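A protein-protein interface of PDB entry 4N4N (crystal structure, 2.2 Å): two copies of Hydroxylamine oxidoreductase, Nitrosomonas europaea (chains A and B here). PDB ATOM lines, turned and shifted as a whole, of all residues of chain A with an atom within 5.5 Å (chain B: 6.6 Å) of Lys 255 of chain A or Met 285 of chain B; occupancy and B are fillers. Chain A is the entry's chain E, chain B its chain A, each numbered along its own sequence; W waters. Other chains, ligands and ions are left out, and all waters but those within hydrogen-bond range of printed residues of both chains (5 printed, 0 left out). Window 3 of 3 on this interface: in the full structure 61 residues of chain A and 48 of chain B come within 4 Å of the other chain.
Lys 255 of chain A touches just one residue of chain B: Met 285 (3.0 Å). Of chain A, only Glu 252 (3.6 Å), Lys 255 (3.0 Å), Glu 257 (3.6 Å) and Ala 258 (3.9 Å) come within 4 Å of Met 285 of chain B. Printed residues of chain B within 4 Å of Glu 257 of chain A: Lys 281 (3.4 Å), Glu 284 (3.7 Å) and Met 285 (3.6 Å). Printed residues of chain A within 4 Å of Leu 282 of chain B: Glu 252. Printed residues of chain A within 4 Å of Lys 278 of chain B: Ala 258. Printed residues of chain B within 4 Å of Ala 258 of chain A: Lys 278 and Met 285. Lys 289 of chain B touches none of the printed residues of chain A. The nearest residue of chain B that does not touch Lys 255 of chain A is Asn 286 of chain B (5.1 Å).
Water W4 bridges NZ of Lys 278 of chain B (2.6 Å) and OE2 of Glu 252 of chain A (2.7 Å). Water W1 lies within hydrogen-bond range of the backbone carbonyl oxygen (O) of Glu 257 of chain A and the side-chain amino group (NZ) of Lys 278 of chain B. Water W2 lies within hydrogen-bond range of NZ of Lys 255 of chain A (2.7 Å), OD1 of Asn 286 of chain B (3.1 Å) and O of Met 285 of chain B (3.4 Å). Water W5 bridges OE2 of Glu 257 of chain A (2.7 Å) and OE1 of Glu 284 of chain B (2.8 Å). Water W3 lies within hydrogen-bond range of the side-chain carboxylate (OE1) of Glu 252 of chain A (2.7 Å) and the side-chain amide nitrogen (ND2) of Asn 286 of chain B (3.2 Å).
No position is printed for both chains. Of the 8 pairs that touch across the chains among the printed residues, none has its exchanged pair printed and touching as well.
Along chain A the printed residues that touch a printed residue of chain B span positions 252 to 258. Of the 11 printed residues of chain B, 5 touch a printed residue of chain A. Printed residues of chain B that touch a printed residue of chain A: Lys 278, Lys 281, Leu 282, Glu 284 and Met 285. Among the printed residues, 8 pairs touch across the chains. Among the printed residues, no Asp or Glu carboxylate lies within 4 Å of a Lys or Arg side-chain nitrogen of the other chain.
The side-chain amino group (NZ) of Lys 278 of chain B lies within hydrogen-bond range of the backbone carbonyl oxygen (O) of Ala 258 of chain A (2.9 Å). O of Glu 252 of chain A sits close to SD of Met 285 of chain B. The backbone carbonyl oxygen (O) of Met 285 of chain B is in hydrogen-bond range of the side-chain amino group (NZ) of Lys 255 of chain A (3.0 Å).
Glu 252 of chain A touches Leu 282 of chain B. O of Glu 257 of chain A touches CD of Lys 281 of chain B, 3.4 Å away. Glu 257 of chain A touches Glu 284 of chain B. Glu 257 of chain A touches Met 285 of chain B. Ala 258 of chain A touches Met 285 of chain B (N to SD, 3.9 Å).
The backbone carbonyl oxygen (O) of Leu 282 of chain B sits close to the side-chain amide nitrogen (ND2) of Asn 286 of chain B (3.2 Å). The backbone carbonyl oxygen (O) of Glu 284 of chain B sits close to the guanidinium group (NE) of Arg 287 of chain B (3.4 Å). OE1 of Glu 284 of chain B is in salt-bridge range of NZ of Lys 281 of chain B (2.9 Å).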
ATOM      1  N   ALA A 250     -18.483  22.685   5.019  1.00  0.00           N
ATOM      2  CA  ALA A 250     -17.808  21.780   5.954  1.00  0.00           C
ATOM      3  C   ALA A 250     -17.405  20.476   5.270  1.00  0.00           C
ATOM      4  O   ALA A 250     -16.335  19.924   5.553  1.00  0.00           O
ATOM      5  CB  ALA A 250     -18.695  21.491   7.162  1.00  0.00           C
ATOM      6  N   ALA A 251     -18.272  19.992   4.378  1.00  0.00           N
ATOM      7  CA  ALA A 251     -18.015  18.779   3.599  1.00  0.00           C
ATOM      8  C   ALA A 251     -16.729  18.909   2.791  1.00  0.00           C
ATOM      9  O   ALA A 251     -15.934  17.974   2.722  1.00  0.00           O
ATOM     10  CB  ALA A 251     -19.200  18.469   2.680  1.00  0.00           C
ATOM     11  N   GLU A 252     -16.532  20.077   2.188  1.00  0.00           N
ATOM     12  CA  GLU A 252     -15.309  20.379   1.446  1.00  0.00           C
ATOM     13  C   GLU A 252     -14.056  20.237   2.324  1.00  0.00           C
ATOM     14  O   GLU A 252     -13.068  19.617   1.912  1.00  0.00           O
ATOM     15  CB  GLU A 252     -15.397  21.784   0.853  1.00  0.00           C
ATOM     16  CG  GLU A 252     -14.154  22.238   0.110  1.00  0.00           C
ATOM     17  CD  GLU A 252     -14.190  23.711  -0.231  1.00  0.00           C
ATOM     18  OE1 GLU A 252     -15.213  24.180  -0.771  1.00  0.00           O
ATOM     19  OE2 GLU A 252     -13.186  24.402   0.029  1.00  0.00           O
ATOM     20  N   SER A 253     -14.111  20.799   3.532  1.00  0.00           N
ATOM     21  CA  SER A 253     -12.971  20.785   4.456  1.00  0.00           C
ATOM     22  C   SER A 253     -12.647  19.393   4.991  1.00  0.00           C
ATOM     23  O   SER A 253     -11.530  19.147   5.459  1.00  0.00           O
ATOM     24  CB  SER A 253     -13.179  21.776   5.607  1.00  0.00           C
ATOM     25  OG  SER A 253     -14.442  21.610   6.224  1.00  0.00           O
ATOM     26  N   ARG A 254     -13.617  18.488   4.905  1.00  0.00           N
ATOM     27  CA  ARG A 254     -13.426  17.093   5.310  1.00  0.00           C
ATOM     28  C   ARG A 254     -12.682  16.271   4.252  1.00  0.00           C
ATOM     29  O   ARG A 254     -12.137  15.201   4.549  1.00  0.00           O
ATOM     30  CB  ARG A 254     -14.774  16.442   5.635  1.00  0.00           C
ATOM     31  CG  ARG A 254     -15.458  17.014   6.868  1.00  0.00           C
ATOM     32  CD  ARG A 254     -16.758  16.282   7.200  1.00  0.00           C
ATOM     33  NE  ARG A 254     -17.494  16.987   8.249  1.00  0.00           N
ATOM     34  CZ  ARG A 254     -18.575  17.736   8.048  1.00  0.00           C
ATOM     35  NH1 ARG A 254     -19.096  17.868   6.830  1.00  0.00           N
ATOM     36  NH2 ARG A 254     -19.152  18.344   9.078  1.00  0.00           N
ATOM     37  N   LYS A 255     -12.661  16.773   3.022  1.00  0.00           N
ATOM     38  CA  LYS A 255     -11.999  16.087   1.918  1.00  0.00           C
ATOM     39  C   LYS A 255     -10.486  16.300   1.968  1.00  0.00           C
ATOM     40  O   LYS A 255     -10.029  17.404   2.249  1.00  0.00           O
ATOM     41  CB  LYS A 255     -12.568  16.559   0.578  1.00  0.00           C
ATOM     42  CG  LYS A 255     -14.018  16.163   0.362  1.00  0.00           C
ATOM     43  CD  LYS A 255     -14.563  16.730  -0.930  1.00  0.00           C
ATOM     44  CE  LYS A 255     -15.963  16.217  -1.206  1.00  0.00           C
ATOM     45  NZ  LYS A 255     -16.477  16.746  -2.501  1.00  0.00           N
ATOM     46  N   PRO A 256      -9.704  15.238   1.692  1.00  0.00           N
ATOM     47  CA  PRO A 256      -8.231  15.293   1.753  1.00  0.00           C
ATOM     48  C   PRO A 256      -7.617  16.400   0.892  1.00  0.00           C
ATOM     49  O   PRO A 256      -6.571  16.957   1.244  1.00  0.00           O
ATOM     50  CB  PRO A 256      -7.809  13.917   1.229  1.00  0.00           C
ATOM     51  CG  PRO A 256      -8.975  13.031   1.522  1.00  0.00           C
ATOM     52  CD  PRO A 256     -10.183  13.895   1.314  1.00  0.00           C
ATOM     53  N   GLU A 257      -8.274  16.717  -0.222  1.00  0.00           N
ATOM     54  CA  GLU A 257      -7.831  17.777  -1.124  1.00  0.00           C
ATOM     55  C   GLU A 257      -7.742  19.157  -0.452  1.00  0.00           C
ATOM     56  O   GLU A 257      -6.923  19.988  -0.845  1.00  0.00           O
ATOM     57  CB  GLU A 257      -8.749  17.852  -2.347  1.00  0.00           C
ATOM     58  CG  GLU A 257      -8.623  16.678  -3.324  1.00  0.00           C
ATOM     59  CD  GLU A 257      -9.444  15.446  -2.920  1.00  0.00           C
ATOM     60  OE1 GLU A 257     -10.204  15.501  -1.929  1.00  0.00           O
ATOM     61  OE2 GLU A 257      -9.327  14.417  -3.610  1.00  0.00           O
ATOM     62  N   ALA A 258      -8.581  19.393   0.556  1.00  0.00           N
ATOM     63  CA  ALA A 258      -8.587  20.668   1.295  1.00  0.00           C
ATOM     64  C   ALA A 258      -7.254  21.001   1.992  1.00  0.00           C
ATOM     65  O   ALA A 258      -6.926  22.178   2.176  1.00  0.00           O
ATOM     66  CB  ALA A 258      -9.735  20.695   2.300  1.00  0.00           C
ATOM     67  N   CYS A 259      -6.497  19.966   2.367  1.00  0.00           N
ATOM     68  CA  CYS A 259      -5.207  20.119   3.059  1.00  0.00           C
ATOM     69  C   CYS A 259      -4.013  20.139   2.099  1.00  0.00           C
ATOM     70  O   CYS A 259      -2.891  20.482   2.493  1.00  0.00           O
ATOM     71  CB  CYS A 259      -4.988  18.972   4.053  1.00  0.00           C
ATOM     72  SG  CYS A 259      -6.439  18.393   4.948  1.00  0.00           S
ATOM     73  N   TRP A 292     -20.144  12.999   2.531  1.00  0.00           N
ATOM     74  CA  TRP A 292     -19.205  13.991   3.058  1.00  0.00           C
ATOM     75  C   TRP A 292     -19.862  15.076   3.925  1.00  0.00           C
ATOM     76  O   TRP A 292     -19.172  15.775   4.671  1.00  0.00           O
ATOM     77  CB  TRP A 292     -18.429  14.649   1.912  1.00  0.00           C
ATOM     78  CG  TRP A 292     -17.514  13.728   1.152  1.00  0.00           C
ATOM     79  CD1 TRP A 292     -17.771  13.119  -0.048  1.00  0.00           C
ATOM     80  CD2 TRP A 292     -16.186  13.329   1.526  1.00  0.00           C
ATOM     81  NE1 TRP A 292     -16.689  12.360  -0.435  1.00  0.00           N
ATOM     82  CE2 TRP A 292     -15.704  12.472   0.512  1.00  0.00           C
ATOM     83  CE3 TRP A 292     -15.361  13.607   2.627  1.00  0.00           C
ATOM     84  CZ2 TRP A 292     -14.434  11.894   0.561  1.00  0.00           C
ATOM     85  CZ3 TRP A 292     -14.095  13.029   2.675  1.00  0.00           C
ATOM     86  CH2 TRP A 292     -13.645  12.183   1.646  1.00  0.00           C
ATOM     87  N   LYS B 278      -5.333  25.940  -4.896  1.00  0.00           N
ATOM     88  CA  LYS B 278      -6.696  25.867  -4.366  1.00  0.00           C
ATOM     89  C   LYS B 278      -7.709  25.754  -5.492  1.00  0.00           C
ATOM     90  O   LYS B 278      -8.659  24.971  -5.400  1.00  0.00           O
ATOM     91  CB  LYS B 278      -7.027  27.080  -3.495  1.00  0.00           C
ATOM     92  CG  LYS B 278      -6.901  26.830  -2.011  1.00  0.00           C
ATOM     93  CD  LYS B 278      -7.925  25.796  -1.526  1.00  0.00           C
ATOM     94  CE  LYS B 278      -7.592  25.387  -0.110  1.00  0.00           C
ATOM     95  NZ  LYS B 278      -8.132  24.054   0.255  1.00  0.00           N
ATOM     96  N   GLY B 280      -7.449  24.337  -8.403  1.00  0.00           N
ATOM     97  CA  GLY B 280      -7.475  22.976  -8.935  1.00  0.00           C
ATOM     98  C   GLY B 280      -8.017  21.939  -7.974  1.00  0.00           C
ATOM     99  O   GLY B 280      -8.715  21.009  -8.382  1.00  0.00           O
ATOM    100  N   LYS B 281      -7.698  22.098  -6.693  1.00  0.00           N
ATOM    101  CA  LYS B 281      -8.194  21.193  -5.658  1.00  0.00           C
ATOM    102  C   LYS B 281      -9.710  21.299  -5.496  1.00  0.00           C
ATOM    103  O   LYS B 281     -10.393  20.288  -5.297  1.00  0.00           O
ATOM    104  CB  LYS B 281      -7.466  21.432  -4.334  1.00  0.00           C
ATOM    105  CG  LYS B 281      -6.052  20.834  -4.300  1.00  0.00           C
ATOM    106  CD  LYS B 281      -6.092  19.317  -4.089  1.00  0.00           C
ATOM    107  CE  LYS B 281      -4.791  18.625  -4.489  1.00  0.00           C
ATOM    108  NZ  LYS B 281      -4.679  18.388  -5.955  1.00  0.00           N
ATOM    109  N   LEU B 282     -10.220  22.526  -5.599  1.00  0.00           N
ATOM    110  CA  LEU B 282     -11.656  22.785  -5.618  1.00  0.00           C
ATOM    111  C   LEU B 282     -12.320  22.206  -6.858  1.00  0.00           C
ATOM    112  O   LEU B 282     -13.417  21.670  -6.772  1.00  0.00           O
ATOM    113  CB  LEU B 282     -11.942  24.288  -5.538  1.00  0.00           C
ATOM    114  CG  LEU B 282     -11.889  24.898  -4.142  1.00  0.00           C
ATOM    115  CD1 LEU B 282     -11.791  26.411  -4.233  1.00  0.00           C
ATOM    116  CD2 LEU B 282     -13.117  24.470  -3.347  1.00  0.00           C
ATOM    117  N   ALA B 283     -11.655  22.325  -8.007  1.00  0.00           N
ATOM    118  CA  ALA B 283     -12.129  21.705  -9.243  1.00  0.00           C
ATOM    119  C   ALA B 283     -12.231  20.189  -9.089  1.00  0.00           C
ATOM    120  O   ALA B 283     -13.196  19.586  -9.555  1.00  0.00           O
ATOM    121  CB  ALA B 283     -11.226  22.064 -10.413  1.00  0.00           C
ATOM    122  N   GLU B 284     -11.234  19.589  -8.432  1.00  0.00           N
ATOM    123  CA  GLU B 284     -11.250  18.157  -8.116  1.00  0.00           C
ATOM    124  C   GLU B 284     -12.412  17.811  -7.169  1.00  0.00           C
ATOM    125  O   GLU B 284     -13.143  16.852  -7.407  1.00  0.00           O
ATOM    126  CB  GLU B 284      -9.896  17.699  -7.535  1.00  0.00           C
ATOM    127  CG  GLU B 284      -8.748  17.673  -8.562  1.00  0.00           C
ATOM    128  CD  GLU B 284      -7.364  17.366  -7.973  1.00  0.00           C
ATOM    129  OE1 GLU B 284      -7.217  17.232  -6.736  1.00  0.00           O
ATOM    130  OE2 GLU B 284      -6.403  17.258  -8.769  1.00  0.00           O
ATOM    131  N   MET B 285     -12.589  18.616  -6.122  1.00  0.00           N
ATOM    132  CA  MET B 285     -13.636  18.386  -5.116  1.00  0.00           C
ATOM    133  C   MET B 285     -15.064  18.637  -5.606  1.00  0.00           C
ATOM    134  O   MET B 285     -15.998  17.960  -5.166  1.00  0.00           O
ATOM    135  CB  MET B 285     -13.366  19.218  -3.855  1.00  0.00           C
ATOM    136  CG  MET B 285     -12.205  18.695  -3.006  1.00  0.00           C
ATOM    137  SD  MET B 285     -11.916  19.598  -1.468  1.00  0.00           S
ATOM    138  CE  MET B 285     -11.162  21.116  -2.065  1.00  0.00           C
ATOM    139  N   ASN B 286     -15.226  19.602  -6.512  1.00  0.00           N
ATOM    140  CA  ASN B 286     -16.551  20.072  -6.938  1.00  0.00           C
ATOM    141  C   ASN B 286     -17.020  19.605  -8.318  1.00  0.00           C
ATOM    142  O   ASN B 286     -18.108  19.983  -8.760  1.00  0.00           O
ATOM    143  CB  ASN B 286     -16.610  21.605  -6.883  1.00  0.00           C
ATOM    144  CG  ASN B 286     -16.412  22.155  -5.477  1.00  0.00           C
ATOM    145  OD1 ASN B 286     -16.784  21.522  -4.487  1.00  0.00           O
ATOM    146  ND2 ASN B 286     -15.830  23.343  -5.388  1.00  0.00           N
ATOM    147  N   ARG B 287     -16.210  18.791  -8.991  1.00  0.00           N
ATOM    148  CA  ARG B 287     -16.499  18.375 -10.367  1.00  0.00           C
ATOM    149  C   ARG B 287     -17.875  17.726 -10.585  1.00  0.00           C
ATOM    150  O   ARG B 287     -18.480  17.908 -11.642  1.00  0.00           O
ATOM    151  CB  ARG B 287     -15.390  17.477 -10.924  1.00  0.00           C
ATOM    152  CG  ARG B 287     -15.043  16.276 -10.068  1.00  0.00           C
ATOM    153  CD  ARG B 287     -14.196  15.291 -10.851  1.00  0.00           C
ATOM    154  NE  ARG B 287     -13.256  14.592  -9.984  1.00  0.00           N
ATOM    155  CZ  ARG B 287     -11.933  14.729 -10.033  1.00  0.00           C
ATOM    156  NH1 ARG B 287     -11.364  15.531 -10.927  1.00  0.00           N
ATOM    157  NH2 ARG B 287     -11.176  14.045  -9.188  1.00  0.00           N
ATOM    158  N   ASP B 288     -18.358  16.985  -9.588  1.00  0.00           N
ATOM    159  CA  ASP B 288     -19.660  16.315  -9.678  1.00  0.00           C
ATOM    160  C   ASP B 288     -20.837  17.253  -9.463  1.00  0.00           C
ATOM    161  O   ASP B 288     -21.967  16.916  -9.814  1.00  0.00           O
ATOM    162  CB  ASP B 288     -19.750  15.165  -8.680  1.00  0.00           C
ATOM    163  CG  ASP B 288     -18.617  14.193  -8.823  1.00  0.00           C
ATOM    164  OD1 ASP B 288     -18.266  13.563  -7.803  1.00  0.00           O
ATOM    165  OD2 ASP B 288     -18.062  14.088  -9.944  1.00  0.00           O
ATOM    166  N   LYS B 289     -20.579  18.417  -8.878  1.00  0.00           N
ATOM    167  CA  LYS B 289     -21.646  19.385  -8.629  1.00  0.00           C
ATOM    168  C   LYS B 289     -21.879  20.295  -9.832  1.00  0.00           C
ATOM    169  O   LYS B 289     -22.907  20.966  -9.919  1.00  0.00           O
ATOM    170  CB  LYS B 289     -21.362  20.199  -7.362  1.00  0.00           C
ATOM    171  CG  LYS B 289     -21.415  19.365  -6.083  1.00  0.00           C
ATOM    172  CD  LYS B 289     -21.312  20.230  -4.835  1.00  0.00           C
ATOM    173  CE  LYS B 289     -21.188  19.379  -3.568  1.00  0.00           C
ATOM    174  NZ  LYS B 289     -22.423  18.595  -3.263  1.00  0.00           N
HETATM  175  O   HOH W   1      -6.393  22.565  -1.321  1.00  0.00           O
HETATM  176  O   HOH W   2     -16.763  19.401  -2.170  1.00  0.00           O
HETATM  177  O   HOH W   3     -16.356  25.401  -2.930  1.00  0.00           O
HETATM  178  O   HOH W   4     -10.650  23.447   0.396  1.00  0.00           O
HETATM  179  O   HOH W   5      -7.841  14.658  -5.874  1.00  0.00           O
